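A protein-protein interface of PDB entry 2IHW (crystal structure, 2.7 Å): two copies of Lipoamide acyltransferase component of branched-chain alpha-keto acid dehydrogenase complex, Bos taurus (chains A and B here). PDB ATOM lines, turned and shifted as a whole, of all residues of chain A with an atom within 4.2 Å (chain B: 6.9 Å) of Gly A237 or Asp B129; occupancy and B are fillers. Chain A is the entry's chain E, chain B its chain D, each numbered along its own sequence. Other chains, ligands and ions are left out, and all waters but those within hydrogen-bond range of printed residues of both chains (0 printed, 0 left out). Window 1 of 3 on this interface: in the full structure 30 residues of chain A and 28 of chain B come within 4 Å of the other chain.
Printed residues of chain A that touch a printed residue of chain B: His A232, Asp A236, Gly A237, Ala A238 and Ser A241. Of the 14 printed residues of chain B, 3 touch a printed residue of chain A. Printed residues of chain B that touch a printed residue of chain A: Met B43, Asp B129 and Ile B184. Hydrophobic or aromatic side chains of chain B within 4 Å of the printed part of chain A: Met B43 and Ile B184. Among the printed residues, 6 pairs touch across the chains. Among the printed residues, no Asp or Glu carboxylate lies within 4 Å of a Lys or Arg side-chain nitrogen of the other chain.
No position is printed for both chains.
OG1 of Thr A239 lies within hydrogen-bond range of OD1 of Asp A236 (2.5 Å).
ND1 of His A232 lies within hydrogen-bond range of SD of Met B43, at 3.7 Å. The backbone NH of Gly A237 lies within hydrogen-bond range of the side-chain carboxylate of Asp B129, at 3.4 Å. The side-chain carboxylate of Asp B129 lies within hydrogen-bond range of the backbone NH of Ala A238 (2.9 Å).
Among the printed residues, pairs that only touch across the chains: Asp A236 with Asp B129 (3.3 Å), Ser A241 with Ile B184 (3.6 Å) and Asp A236 with Met B43 (3.9 Å).
Of chain B, only Asp B129 comes within 4 Å of Gly A237. Of the printed residues of chain A, Asp B129 touches Asp A236 (3.3 Å), Gly A237 (3.4 Å) and Ala A238 (2.9 Å). Of the printed residues of chain B, Ser A241 touches Ile B184. Printed residues of chain A within 4 Å of Ile B184: Ser A241. Gly B161 touches none of the printed residues of chain A. The nearest printed residue of chain A that does not touch Asp B129 is Thr A239 (5.1 Å).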
ATOM      1  N   PHE A  56      -5.955  30.381  12.263  1.00  0.00           N
ATOM      2  CA  PHE A  56      -5.911  29.234  13.128  1.00  0.00           C
ATOM      3  C   PHE A  56      -6.091  29.722  14.566  1.00  0.00           C
ATOM      4  O   PHE A  56      -5.409  30.656  15.022  1.00  0.00           O
ATOM      5  CB  PHE A  56      -4.586  28.510  12.928  1.00  0.00           C
ATOM      6  CG  PHE A  56      -4.299  27.463  13.937  1.00  0.00           C
ATOM      7  CD1 PHE A  56      -5.084  26.309  14.026  1.00  0.00           C
ATOM      8  CD2 PHE A  56      -3.260  27.618  14.828  1.00  0.00           C
ATOM      9  CE1 PHE A  56      -4.814  25.291  15.029  1.00  0.00           C
ATOM     10  CE2 PHE A  56      -2.959  26.612  15.800  1.00  0.00           C
ATOM     11  CZ  PHE A  56      -3.728  25.448  15.902  1.00  0.00           C
ATOM     12  N   HIS A 232      -2.153  30.793   9.497  1.00  0.00           N
ATOM     13  CA  HIS A 232      -1.608  29.479   9.281  1.00  0.00           C
ATOM     14  C   HIS A 232      -0.817  29.244   7.936  1.00  0.00           C
ATOM     15  O   HIS A 232      -0.284  28.168   7.661  1.00  0.00           O
ATOM     16  CB  HIS A 232      -2.698  28.436   9.506  1.00  0.00           C
ATOM     17  CG  HIS A 232      -2.184  27.172  10.135  1.00  0.00           C
ATOM     18  ND1 HIS A 232      -1.000  26.578   9.752  1.00  0.00           N
ATOM     19  CD2 HIS A 232      -2.677  26.411  11.137  1.00  0.00           C
ATOM     20  CE1 HIS A 232      -0.775  25.525  10.506  1.00  0.00           C
ATOM     21  NE2 HIS A 232      -1.777  25.402  11.356  1.00  0.00           N
ATOM     22  N   ASP A 236       2.802  27.642  12.024  1.00  0.00           N
ATOM     23  CA  ASP A 236       2.214  26.337  12.318  1.00  0.00           C
ATOM     24  C   ASP A 236       1.692  26.285  13.748  1.00  0.00           C
ATOM     25  O   ASP A 236       1.877  27.215  14.520  1.00  0.00           O
ATOM     26  CB  ASP A 236       3.177  25.180  11.983  1.00  0.00           C
ATOM     27  CG  ASP A 236       4.503  25.168  12.845  1.00  0.00           C
ATOM     28  OD1 ASP A 236       4.599  25.782  13.919  1.00  0.00           O
ATOM     29  OD2 ASP A 236       5.484  24.486  12.454  1.00  0.00           O
ATOM     30  N   GLY A 237       1.068  25.175  14.104  1.00  0.00           N
ATOM     31  CA  GLY A 237       0.466  24.947  15.427  1.00  0.00           C
ATOM     32  C   GLY A 237       1.427  24.837  16.584  1.00  0.00           C
ATOM     33  O   GLY A 237       1.180  25.374  17.627  1.00  0.00           O
ATOM     34  N   ALA A 238       2.512  24.123  16.385  1.00  0.00           N
ATOM     35  CA  ALA A 238       3.619  24.075  17.342  1.00  0.00           C
ATOM     36  C   ALA A 238       4.118  25.453  17.727  1.00  0.00           C
ATOM     37  O   ALA A 238       4.398  25.714  18.865  1.00  0.00           O
ATOM     38  CB  ALA A 238       4.792  23.274  16.766  1.00  0.00           C
ATOM     39  N   THR A 239       4.250  26.340  16.767  1.00  0.00           N
ATOM     40  CA  THR A 239       4.815  27.630  17.082  1.00  0.00           C
ATOM     41  C   THR A 239       3.852  28.401  18.009  1.00  0.00           C
ATOM     42  O   THR A 239       4.269  28.946  19.026  1.00  0.00           O
ATOM     43  CB  THR A 239       5.110  28.391  15.809  1.00  0.00           C
ATOM     44  OG1 THR A 239       5.972  27.599  15.027  1.00  0.00           O
ATOM     45  CG2 THR A 239       5.829  29.661  16.112  1.00  0.00           C
ATOM     46  N   VAL A 240       2.566  28.424  17.673  1.00  0.00           N
ATOM     47  CA  VAL A 240       1.654  29.184  18.485  1.00  0.00           C
ATOM     48  C   VAL A 240       1.607  28.632  19.897  1.00  0.00           C
ATOM     49  O   VAL A 240       1.703  29.365  20.889  1.00  0.00           O
ATOM     50  CB  VAL A 240       0.266  29.219  17.894  1.00  0.00           C
ATOM     51  CG1 VAL A 240      -0.752  29.597  18.983  1.00  0.00           C
ATOM     52  CG2 VAL A 240       0.251  30.265  16.852  1.00  0.00           C
ATOM     53  N   SER A 241       1.472  27.325  19.967  1.00  0.00           N
ATOM     54  CA  SER A 241       1.469  26.598  21.203  1.00  0.00           C
ATOM     55  C   SER A 241       2.699  26.798  22.100  1.00  0.00           C
ATOM     56  O   SER A 241       2.572  27.102  23.294  1.00  0.00           O
ATOM     57  CB  SER A 241       1.351  25.146  20.875  1.00  0.00           C
ATOM     58  OG  SER A 241       0.576  24.691  21.929  1.00  0.00           O
ATOM     59  N   MET B  43       2.314  24.665   2.857  1.00  0.00           N
ATOM     60  CA  MET B  43       1.368  25.171   3.832  1.00  0.00           C
ATOM     61  C   MET B  43       0.656  26.430   3.346  1.00  0.00           C
ATOM     62  O   MET B  43      -0.576  26.542   3.509  1.00  0.00           O
ATOM     63  CB  MET B  43       2.014  25.426   5.178  1.00  0.00           C
ATOM     64  CG  MET B  43       1.051  25.454   6.271  1.00  0.00           C
ATOM     65  SD  MET B  43       1.884  25.216   7.830  1.00  0.00           S
ATOM     66  CE  MET B  43       2.733  26.786   8.198  1.00  0.00           C
ATOM     67  N   ALA B 127      -2.027  15.421  12.435  1.00  0.00           N
ATOM     68  CA  ALA B 127      -1.315  16.626  12.058  1.00  0.00           C
ATOM     69  C   ALA B 127      -0.035  16.721  12.873  1.00  0.00           C
ATOM     70  O   ALA B 127      -0.069  16.442  14.038  1.00  0.00           O
ATOM     71  CB  ALA B 127      -2.205  17.814  12.313  1.00  0.00           C
ATOM     72  N   MET B 128       1.084  17.113  12.275  1.00  0.00           N
ATOM     73  CA  MET B 128       2.302  17.327  13.064  1.00  0.00           C
ATOM     74  C   MET B 128       3.168  18.432  12.486  1.00  0.00           C
ATOM     75  O   MET B 128       2.972  18.825  11.331  1.00  0.00           O
ATOM     76  CB  MET B 128       3.159  16.072  13.116  1.00  0.00           C
ATOM     77  CG  MET B 128       2.464  14.788  12.793  1.00  0.00           C
ATOM     78  SD  MET B 128       3.733  13.528  12.532  1.00  0.00           S
ATOM     79  CE  MET B 128       3.189  12.188  13.663  1.00  0.00           C
ATOM     80  N   ASP B 129       4.145  18.913  13.252  1.00  0.00           N
ATOM     81  CA  ASP B 129       5.061  19.891  12.702  1.00  0.00           C
ATOM     82  C   ASP B 129       6.519  19.432  12.828  1.00  0.00           C
ATOM     83  O   ASP B 129       6.909  18.825  13.813  1.00  0.00           O
ATOM     84  CB  ASP B 129       4.810  21.308  13.258  1.00  0.00           C
ATOM     85  CG  ASP B 129       3.324  21.743  13.156  1.00  0.00           C
ATOM     86  OD1 ASP B 129       2.721  21.618  12.052  1.00  0.00           O
ATOM     87  OD2 ASP B 129       2.744  22.227  14.171  1.00  0.00           O
ATOM     88  N   THR B 130       7.299  19.690  11.795  1.00  0.00           N
ATOM     89  CA  THR B 130       8.717  19.402  11.801  1.00  0.00           C
ATOM     90  C   THR B 130       9.341  20.747  11.432  1.00  0.00           C
ATOM     91  O   THR B 130       8.586  21.721  11.265  1.00  0.00           O
ATOM     92  CB  THR B 130       9.058  18.340  10.736  1.00  0.00           C
ATOM     93  OG1 THR B 130       8.791  18.870   9.433  1.00  0.00           O
ATOM     94  CG2 THR B 130       8.228  17.098  10.917  1.00  0.00           C
ATOM     95  N   GLU B 131      10.666  20.861  11.293  1.00  0.00           N
ATOM     96  CA  GLU B 131      11.177  22.189  10.885  1.00  0.00           C
ATOM     97  C   GLU B 131      10.754  22.494   9.458  1.00  0.00           C
ATOM     98  O   GLU B 131      10.652  23.671   9.066  1.00  0.00           O
ATOM     99  CB  GLU B 131      12.684  22.466  11.135  1.00  0.00           C
ATOM    100  CG  GLU B 131      13.657  21.326  10.837  1.00  0.00           C
ATOM    101  CD  GLU B 131      13.600  20.217  11.898  1.00  0.00           C
ATOM    102  OE1 GLU B 131      14.259  19.161  11.691  1.00  0.00           O
ATOM    103  OE2 GLU B 131      12.897  20.408  12.931  1.00  0.00           O
ATOM    104  N   GLN B 132      10.453  21.439   8.704  1.00  0.00           N
ATOM    105  CA  GLN B 132       9.772  21.619   7.426  1.00  0.00           C
ATOM    106  C   GLN B 132       8.314  22.120   7.557  1.00  0.00           C
ATOM    107  O   GLN B 132       7.716  22.504   6.558  1.00  0.00           O
ATOM    108  CB  GLN B 132       9.809  20.324   6.584  1.00  0.00           C
ATOM    109  CG  GLN B 132      10.825  20.308   5.442  1.00  0.00           C
ATOM    110  CD  GLN B 132      12.215  19.912   5.893  1.00  0.00           C
ATOM    111  OE1 GLN B 132      12.480  18.740   6.172  1.00  0.00           O
ATOM    112  NE2 GLN B 132      13.118  20.889   5.953  1.00  0.00           N
ATOM    113  N   GLY B 133       7.726  22.100   8.751  1.00  0.00           N
ATOM    114  CA  GLY B 133       6.333  22.558   8.888  1.00  0.00           C
ATOM    115  C   GLY B 133       5.233  21.511   8.997  1.00  0.00           C
ATOM    116  O   GLY B 133       5.454  20.390   9.467  1.00  0.00           O
ATOM    117  N   LEU B 134       4.032  21.883   8.557  1.00  0.00           N
ATOM    118  CA  LEU B 134       2.847  21.015   8.676  1.00  0.00           C
ATOM    119  C   LEU B 134       3.009  19.765   7.859  1.00  0.00           C
ATOM    120  O   LEU B 134       3.415  19.821   6.707  1.00  0.00           O
ATOM    121  CB  LEU B 134       1.574  21.737   8.237  1.00  0.00           C
ATOM    122  CG  LEU B 134       0.234  20.989   8.271  1.00  0.00           C
ATOM    123  CD1 LEU B 134      -0.228  20.634   9.627  1.00  0.00           C
ATOM    124  CD2 LEU B 134      -0.849  21.798   7.550  1.00  0.00           C
ATOM    125  N   ILE B 135       2.681  18.638   8.463  1.00  0.00           N
ATOM    126  CA  ILE B 135       2.803  17.366   7.795  1.00  0.00           C
ATOM    127  C   ILE B 135       1.727  16.459   8.410  1.00  0.00           C
ATOM    128  O   ILE B 135       1.564  16.389   9.631  1.00  0.00           O
ATOM    129  CB  ILE B 135       4.288  16.848   7.863  1.00  0.00           C
ATOM    130  CG1 ILE B 135       4.482  15.600   7.036  1.00  0.00           C
ATOM    131  CG2 ILE B 135       4.804  16.687   9.252  1.00  0.00           C
ATOM    132  CD1 ILE B 135       5.067  15.903   5.646  1.00  0.00           C
ATOM    133  N   GLY B 161       8.061  10.391  10.372  1.00  0.00           N
ATOM    134  CA  GLY B 161       7.830  11.814  10.323  1.00  0.00           C
ATOM    135  C   GLY B 161       8.996  12.646  10.835  1.00  0.00           C
ATOM    136  O   GLY B 161       9.408  13.616  10.167  1.00  0.00           O
ATOM    137  N   SER B 179      -5.774  16.588  15.287  1.00  0.00           N
ATOM    138  CA  SER B 179      -4.566  17.285  15.632  1.00  0.00           C
ATOM    139  C   SER B 179      -4.492  17.353  17.121  1.00  0.00           C
ATOM    140  O   SER B 179      -5.369  17.943  17.759  1.00  0.00           O
ATOM    141  CB  SER B 179      -4.555  18.678  15.074  1.00  0.00           C
ATOM    142  OG  SER B 179      -3.282  19.226  15.350  1.00  0.00           O
ATOM    143  N   ILE B 181      -3.109  19.004  19.694  1.00  0.00           N
ATOM    144  CA  ILE B 181      -2.461  20.231  20.122  1.00  0.00           C
ATOM    145  C   ILE B 181      -2.009  20.125  21.597  1.00  0.00           C
ATOM    146  O   ILE B 181      -1.013  20.735  22.026  1.00  0.00           O
ATOM    147  CB  ILE B 181      -3.428  21.479  19.900  1.00  0.00           C
ATOM    148  CG1 ILE B 181      -4.589  21.506  20.925  1.00  0.00           C
ATOM    149  CG2 ILE B 181      -3.949  21.562  18.447  1.00  0.00           C
ATOM    150  CD1 ILE B 181      -5.268  22.875  21.088  1.00  0.00           C
ATOM    151  N   ILE B 184       1.216  19.535  23.292  1.00  0.00           N
ATOM    152  CA  ILE B 184       2.033  20.644  23.734  1.00  0.00           C
ATOM    153  C   ILE B 184       1.325  21.494  24.799  1.00  0.00           C
ATOM    154  O   ILE B 184       1.928  21.802  25.837  1.00  0.00           O
ATOM    155  CB  ILE B 184       2.526  21.473  22.551  1.00  0.00           C
ATOM    156  CG1 ILE B 184       3.347  20.565  21.619  1.00  0.00           C
ATOM    157  CG2 ILE B 184       3.347  22.681  23.043  1.00  0.00           C
ATOM    158  CD1 ILE B 184       3.670  21.104  20.255  1.00  0.00           C
